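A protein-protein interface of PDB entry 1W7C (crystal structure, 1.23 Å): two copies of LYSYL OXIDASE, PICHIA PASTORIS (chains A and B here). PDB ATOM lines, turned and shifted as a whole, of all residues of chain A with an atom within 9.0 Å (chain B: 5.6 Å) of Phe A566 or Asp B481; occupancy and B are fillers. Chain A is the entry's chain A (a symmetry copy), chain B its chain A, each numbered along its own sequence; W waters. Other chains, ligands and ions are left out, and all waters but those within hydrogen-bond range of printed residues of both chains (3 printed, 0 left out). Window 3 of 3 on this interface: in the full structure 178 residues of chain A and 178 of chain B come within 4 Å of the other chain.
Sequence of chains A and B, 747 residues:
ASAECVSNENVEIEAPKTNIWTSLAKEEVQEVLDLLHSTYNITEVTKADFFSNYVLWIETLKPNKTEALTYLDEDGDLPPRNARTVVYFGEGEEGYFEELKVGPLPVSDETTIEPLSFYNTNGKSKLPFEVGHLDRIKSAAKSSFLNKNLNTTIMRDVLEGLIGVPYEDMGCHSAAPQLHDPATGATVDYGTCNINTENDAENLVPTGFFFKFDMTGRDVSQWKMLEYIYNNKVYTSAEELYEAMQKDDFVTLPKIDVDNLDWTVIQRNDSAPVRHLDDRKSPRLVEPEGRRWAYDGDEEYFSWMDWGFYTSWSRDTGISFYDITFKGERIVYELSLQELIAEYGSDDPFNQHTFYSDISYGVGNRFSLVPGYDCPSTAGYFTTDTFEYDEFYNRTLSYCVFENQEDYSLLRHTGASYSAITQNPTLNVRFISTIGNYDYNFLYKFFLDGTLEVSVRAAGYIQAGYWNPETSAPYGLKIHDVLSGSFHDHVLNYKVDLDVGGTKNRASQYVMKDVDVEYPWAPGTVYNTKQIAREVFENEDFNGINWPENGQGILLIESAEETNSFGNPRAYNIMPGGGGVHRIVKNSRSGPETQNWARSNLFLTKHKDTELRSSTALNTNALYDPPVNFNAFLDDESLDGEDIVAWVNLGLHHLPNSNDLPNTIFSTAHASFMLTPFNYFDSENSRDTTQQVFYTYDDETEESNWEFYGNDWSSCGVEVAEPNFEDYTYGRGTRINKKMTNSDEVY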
ATOM      1  N   THR A 563      13.369  26.510   5.755  1.00  0.00           N
ATOM      2  CA  THR A 563      12.714  27.021   4.556  1.00  0.00           C
ATOM      3  C   THR A 563      12.542  25.917   3.544  1.00  0.00           C
ATOM      4  O   THR A 563      13.221  24.893   3.625  1.00  0.00           O
ATOM      5  CB  THR A 563      13.543  28.163   3.928  1.00  0.00           C
ATOM      6  OG1 THR A 563      14.849  27.677   3.571  1.00  0.00           O
ATOM      7  CG2 THR A 563      13.782  29.312   4.901  1.00  0.00           C
ATOM      8  N   ASN A 564      11.678  26.154   2.562  1.00  0.00           N
ATOM      9  CA  ASN A 564      11.631  25.307   1.387  1.00  0.00           C
ATOM     10  C   ASN A 564      12.698  25.753   0.382  1.00  0.00           C
ATOM     11  O   ASN A 564      13.552  26.621   0.701  1.00  0.00           O
ATOM     12  CB  ASN A 564      10.201  25.191   0.811  1.00  0.00           C
ATOM     13  CG  ASN A 564       9.748  26.393   0.020  1.00  0.00           C
ATOM     14  OD1 ASN A 564      10.474  27.384  -0.151  1.00  0.00           O
ATOM     15  ND2 ASN A 564       8.509  26.318  -0.470  1.00  0.00           N
ATOM     16  N   SER A 565      12.718  25.097  -0.772  1.00  0.00           N
ATOM     17  CA  SER A 565      13.820  25.276  -1.716  1.00  0.00           C
ATOM     18  C   SER A 565      13.859  26.668  -2.324  1.00  0.00           C
ATOM     19  O   SER A 565      14.881  27.060  -2.876  1.00  0.00           O
ATOM     20  CB  SER A 565      13.765  24.219  -2.819  1.00  0.00           C
ATOM     21  OG  SER A 565      13.942  22.941  -2.255  1.00  0.00           O
ATOM     22  N   PHE A 566      12.758  27.409  -2.216  1.00  0.00           N
ATOM     23  CA  PHE A 566      12.668  28.757  -2.789  1.00  0.00           C
ATOM     24  C   PHE A 566      12.803  29.864  -1.759  1.00  0.00           C
ATOM     25  O   PHE A 566      12.570  31.023  -2.054  1.00  0.00           O
ATOM     26  CB  PHE A 566      11.393  28.854  -3.626  1.00  0.00           C
ATOM     27  CG  PHE A 566      11.246  27.693  -4.529  1.00  0.00           C
ATOM     28  CD1 PHE A 566      10.294  26.720  -4.286  1.00  0.00           C
ATOM     29  CD2 PHE A 566      12.176  27.469  -5.527  1.00  0.00           C
ATOM     30  CE1 PHE A 566      10.236  25.587  -5.044  1.00  0.00           C
ATOM     31  CE2 PHE A 566      12.117  26.310  -6.305  1.00  0.00           C
ATOM     32  CZ  PHE A 566      11.132  25.386  -6.072  1.00  0.00           C
ATOM     33  N   GLY A 567      13.239  29.495  -0.561  1.00  0.00           N
ATOM     34  CA  GLY A 567      13.587  30.461   0.463  1.00  0.00           C
ATOM     35  C   GLY A 567      12.446  30.856   1.375  1.00  0.00           C
ATOM     36  O   GLY A 567      12.628  31.654   2.261  1.00  0.00           O
ATOM     37  N   ASN A 568      11.267  30.272   1.183  1.00  0.00           N
ATOM     38  CA  ASN A 568      10.119  30.625   2.006  1.00  0.00           C
ATOM     39  C   ASN A 568      10.142  29.824   3.303  1.00  0.00           C
ATOM     40  O   ASN A 568      10.347  28.613   3.261  1.00  0.00           O
ATOM     41  CB  ASN A 568       8.815  30.325   1.251  1.00  0.00           C
ATOM     42  CG  ASN A 568       8.668  31.153  -0.007  1.00  0.00           C
ATOM     43  OD1 ASN A 568       8.772  32.389   0.037  1.00  0.00           O
ATOM     44  ND2 ASN A 568       8.536  30.486  -1.145  1.00  0.00           N
ATOM     45  N   PRO A 569       9.876  30.465   4.433  1.00  0.00           N
ATOM     46  CA  PRO A 569       9.690  29.712   5.672  1.00  0.00           C
ATOM     47  C   PRO A 569       8.659  28.588   5.511  1.00  0.00           C
ATOM     48  O   PRO A 569       7.560  28.798   4.973  1.00  0.00           O
ATOM     49  CB  PRO A 569       9.191  30.771   6.644  1.00  0.00           C
ATOM     50  CG  PRO A 569       9.771  32.090   6.161  1.00  0.00           C
ATOM     51  CD  PRO A 569       9.700  31.914   4.635  1.00  0.00           C
ATOM     52  N   ARG A 570       8.982  27.405   5.984  1.00  0.00           N
ATOM     53  CA  ARG A 570       7.997  26.335   6.008  1.00  0.00           C
ATOM     54  C   ARG A 570       6.877  26.773   6.944  1.00  0.00           C
ATOM     55  O   ARG A 570       7.136  27.241   8.043  1.00  0.00           O
ATOM     56  CB  ARG A 570       8.628  25.060   6.551  1.00  0.00           C
ATOM     57  CG  ARG A 570       9.742  24.508   5.689  1.00  0.00           C
ATOM     58  CD  ARG A 570      10.259  23.203   6.164  1.00  0.00           C
ATOM     59  NE  ARG A 570       9.333  22.160   5.813  1.00  0.00           N
ATOM     60  CZ  ARG A 570       9.393  20.921   6.290  1.00  0.00           C
ATOM     61  NH1 ARG A 570      10.300  20.577   7.188  1.00  0.00           N
ATOM     62  NH2 ARG A 570       8.559  20.029   5.849  1.00  0.00           N
ATOM     63  N   ASN A 679       3.829  26.692   1.843  1.00  0.00           N
ATOM     64  CA  ASN A 679       5.280  26.633   1.643  1.00  0.00           C
ATOM     65  C   ASN A 679       5.988  25.619   2.539  1.00  0.00           C
ATOM     66  O   ASN A 679       7.181  25.687   2.749  1.00  0.00           O
ATOM     67  CB  ASN A 679       5.892  28.043   1.764  1.00  0.00           C
ATOM     68  CG  ASN A 679       5.392  28.960   0.700  1.00  0.00           C
ATOM     69  OD1 ASN A 679       5.087  28.545  -0.419  1.00  0.00           O
ATOM     70  ND2 ASN A 679       5.340  30.238   1.028  1.00  0.00           N
ATOM     71  N   PHE A 681       6.195  22.378   1.946  1.00  0.00           N
ATOM     72  CA  PHE A 681       6.946  21.610   0.976  1.00  0.00           C
ATOM     73  C   PHE A 681       7.340  22.513  -0.195  1.00  0.00           C
ATOM     74  O   PHE A 681       6.978  23.688  -0.239  1.00  0.00           O
ATOM     75  CB  PHE A 681       6.104  20.429   0.487  1.00  0.00           C
ATOM     76  CG  PHE A 681       5.646  19.470   1.576  1.00  0.00           C
ATOM     77  CD1 PHE A 681       6.549  18.690   2.294  1.00  0.00           C
ATOM     78  CD2 PHE A 681       4.278  19.268   1.808  1.00  0.00           C
ATOM     79  CE1 PHE A 681       6.107  17.809   3.252  1.00  0.00           C
ATOM     80  CE2 PHE A 681       3.837  18.342   2.758  1.00  0.00           C
ATOM     81  CZ  PHE A 681       4.748  17.612   3.456  1.00  0.00           C
ATOM     82  N   ASP A 682       8.014  21.950  -1.186  1.00  0.00           N
ATOM     83  CA  ASP A 682       8.241  22.618  -2.445  1.00  0.00           C
ATOM     84  C   ASP A 682       7.041  22.558  -3.393  1.00  0.00           C
ATOM     85  O   ASP A 682       6.975  23.322  -4.353  1.00  0.00           O
ATOM     86  CB  ASP A 682       9.449  21.999  -3.157  1.00  0.00           C
ATOM     87  CG  ASP A 682      10.758  22.293  -2.487  1.00  0.00           C
ATOM     88  OD1 ASP A 682      10.826  23.176  -1.611  1.00  0.00           O
ATOM     89  OD2 ASP A 682      11.785  21.677  -2.866  1.00  0.00           O
ATOM     90  N   SER A 683       6.122  21.648  -3.125  1.00  0.00           N
ATOM     91  CA  SER A 683       4.992  21.393  -3.987  1.00  0.00           C
ATOM     92  C   SER A 683       3.853  20.774  -3.170  1.00  0.00           C
ATOM     93  O   SER A 683       4.014  20.397  -2.002  1.00  0.00           O
ATOM     94  CB  SER A 683       5.409  20.458  -5.127  1.00  0.00           C
ATOM     95  OG  SER A 683       5.852  19.215  -4.605  1.00  0.00           O
ATOM     96  N   TRP B 467       9.057  36.080 -11.735  1.00  0.00           N
ATOM     97  CA  TRP B 467       9.579  36.630 -10.491  1.00  0.00           C
ATOM     98  C   TRP B 467      10.779  37.527 -10.748  1.00  0.00           C
ATOM     99  O   TRP B 467      11.863  37.028 -11.091  1.00  0.00           O
ATOM    100  CB  TRP B 467       9.973  35.514  -9.512  1.00  0.00           C
ATOM    101  CG  TRP B 467      10.615  36.047  -8.252  1.00  0.00           C
ATOM    102  CD1 TRP B 467      11.937  36.151  -8.003  1.00  0.00           C
ATOM    103  CD2 TRP B 467       9.950  36.545  -7.079  1.00  0.00           C
ATOM    104  NE1 TRP B 467      12.144  36.687  -6.757  1.00  0.00           N
ATOM    105  CE2 TRP B 467      10.942  36.947  -6.173  1.00  0.00           C
ATOM    106  CE3 TRP B 467       8.606  36.713  -6.710  1.00  0.00           C
ATOM    107  CZ2 TRP B 467      10.652  37.485  -4.903  1.00  0.00           C
ATOM    108  CZ3 TRP B 467       8.322  37.232  -5.454  1.00  0.00           C
ATOM    109  CH2 TRP B 467       9.350  37.628  -4.569  1.00  0.00           C
ATOM    110  N   LYS B 478       7.505  33.967  -4.181  1.00  0.00           N
ATOM    111  CA  LYS B 478       8.370  33.200  -5.063  1.00  0.00           C
ATOM    112  C   LYS B 478       8.162  31.729  -4.806  1.00  0.00           C
ATOM    113  O   LYS B 478       8.515  31.221  -3.743  1.00  0.00           O
ATOM    114  CB  LYS B 478       9.831  33.567  -4.831  1.00  0.00           C
ATOM    115  CG  LYS B 478      10.765  32.940  -5.851  1.00  0.00           C
ATOM    116  CD  LYS B 478      12.222  33.240  -5.497  1.00  0.00           C
ATOM    117  CE  LYS B 478      13.176  32.426  -6.335  1.00  0.00           C
ATOM    118  NZ  LYS B 478      14.590  32.797  -6.040  1.00  0.00           N
ATOM    119  N   ILE B 479       7.546  31.052  -5.764  1.00  0.00           N
ATOM    120  CA  ILE B 479       7.158  29.649  -5.598  1.00  0.00           C
ATOM    121  C   ILE B 479       7.922  28.692  -6.510  1.00  0.00           C
ATOM    122  O   ILE B 479       7.772  27.482  -6.390  1.00  0.00           O
ATOM    123  CB  ILE B 479       5.640  29.469  -5.799  1.00  0.00           C
ATOM    124  CG1 ILE B 479       5.210  29.885  -7.214  1.00  0.00           C
ATOM    125  CG2 ILE B 479       4.878  30.249  -4.704  1.00  0.00           C
ATOM    126  CD1 ILE B 479       3.735  29.575  -7.536  1.00  0.00           C
ATOM    127  N   HIS B 480       8.756  29.237  -7.396  1.00  0.00           N
ATOM    128  CA  HIS B 480       9.703  28.381  -8.107  1.00  0.00           C
ATOM    129  C   HIS B 480      10.866  29.311  -8.508  1.00  0.00           C
ATOM    130  O   HIS B 480      10.852  30.515  -8.179  1.00  0.00           O
ATOM    131  CB  HIS B 480       9.030  27.633  -9.278  1.00  0.00           C
ATOM    132  CG  HIS B 480       9.796  26.428  -9.725  1.00  0.00           C
ATOM    133  ND1 HIS B 480      10.697  26.477 -10.766  1.00  0.00           N
ATOM    134  CD2 HIS B 480       9.809  25.155  -9.272  1.00  0.00           C
ATOM    135  CE1 HIS B 480      11.262  25.286 -10.906  1.00  0.00           C
ATOM    136  NE2 HIS B 480      10.726  24.462 -10.022  1.00  0.00           N
ATOM    137  N   ASP B 481      11.905  28.771  -9.143  1.00  0.00           N
ATOM    138  CA  ASP B 481      13.158  29.506  -9.292  1.00  0.00           C
ATOM    139  C   ASP B 481      12.962  30.897  -9.875  1.00  0.00           C
ATOM    140  O   ASP B 481      13.587  31.847  -9.402  1.00  0.00           O
ATOM    141  CB  ASP B 481      14.137  28.766 -10.218  1.00  0.00           C
ATOM    142  CG  ASP B 481      14.513  27.382  -9.719  1.00  0.00           C
ATOM    143  OD1 ASP B 481      15.729  27.087  -9.657  1.00  0.00           O
ATOM    144  OD2 ASP B 481      13.683  26.511  -9.410  1.00  0.00           O
ATOM    145  N   VAL B 482      12.117  31.024 -10.903  1.00  0.00           N
ATOM    146  CA  VAL B 482      11.820  32.329 -11.494  1.00  0.00           C
ATOM    147  C   VAL B 482      10.320  32.574 -11.623  1.00  0.00           C
ATOM    148  O   VAL B 482       9.868  33.283 -12.534  1.00  0.00           O
ATOM    149  CB  VAL B 482      12.543  32.548 -12.845  1.00  0.00           C
ATOM    150  CG1 VAL B 482      14.048  32.591 -12.621  1.00  0.00           C
ATOM    151  CG2 VAL B 482      12.143  31.514 -13.859  1.00  0.00           C
ATOM    152  N   LEU B 483       9.574  32.094 -10.628  1.00  0.00           N
ATOM    153  CA  LEU B 483       8.112  32.111 -10.689  1.00  0.00           C
ATOM    154  C   LEU B 483       7.507  32.762  -9.456  1.00  0.00           C
ATOM    155  O   LEU B 483       7.859  32.407  -8.334  1.00  0.00           O
ATOM    156  CB  LEU B 483       7.565  30.695 -10.799  1.00  0.00           C
ATOM    157  CG  LEU B 483       6.098  30.566 -11.202  1.00  0.00           C
ATOM    158  CD1 LEU B 483       5.892  31.140 -12.586  1.00  0.00           C
ATOM    159  CD2 LEU B 483       5.586  29.149 -11.143  1.00  0.00           C
HETATM  160  O   HOH W   1       8.687  34.503  -1.592  1.00  0.00           O
HETATM  161  O   HOH W   2       6.736  26.192  -4.276  1.00  0.00           O
HETATM  162  O   HOH W   3      15.091  31.952  -3.417  1.00  0.00           O
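Among the printed residues, pairs that only touch across the chains: Phe A566 with Lys B478 (3.7 Å), Phe A566 with Ile B479 (3.4 Å), Phe A566 with His B480 (3.5 Å) and Phe A566 with Asp B481 (3.5 Å).
Hydrophobic or aromatic side chains of chain A within 4 Å of the printed part of chain B: Phe A566.
Printed residues of chain B that touch a printed residue of chain A: Lys B478, Ile B479, His B480 and Asp B481.
Among the printed residues, 5 pairs touch across the chains.
Water W1 bridges the side-chain amide oxygen (OD1) of Asn A568 (2.7 Å) and the backbone NH (N) of Lys B478 (2.9 Å).
Water W2 bridges the backbone carbonyl oxygen of Ile B479 (2.7 Å) and the backbone carbonyl oxygen of Asp A682 (2.9 Å).
Water W3 lies within hydrogen-bond range of the side-chain amino group of Lys B478 (2.8 Å) and the backbone carbonyl oxygen of Phe A566 (3.0 Å).
ND2 of Asn A568 is in hydrogen-bond range of O of Lys B478 (2.7 Å).
Of the printed residues of chain B, Phe A566 touches Lys B478 (3.7 Å), Ile B479 (3.4 Å), His B480 (3.5 Å) and Asp B481 (3.5 Å).
Printed residues of chain B within 4 Å of Asn A568: Lys B478.
Phe A681 touches none of the printed residues of chain B.
Of the printed residues of chain A, Lys B478 touches Phe A566 (3.7 Å) and Asn A568 (2.7 Å).
Printed residues of chain A within 4 Å of Ile B479: Phe A566.
Of chain A, only Phe A566 comes within 4 Å of His B480.
The side-chain amide oxygen of Asn A564 lies within hydrogen-bond range of the backbone NH of Asn A568.
The side-chain carboxylate (OD2) of Asp B481 lies close to a ring nitrogen (ND1) of His B480.
The backbone NH of Phe A566 sits at hydrogen-bond distance from the side-chain amide oxygen of Asn A564.
No position is printed for both chains.
Of the 5 pairs that touch across the chains among the printed residues, none has its exchanged pair printed and touching as well.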
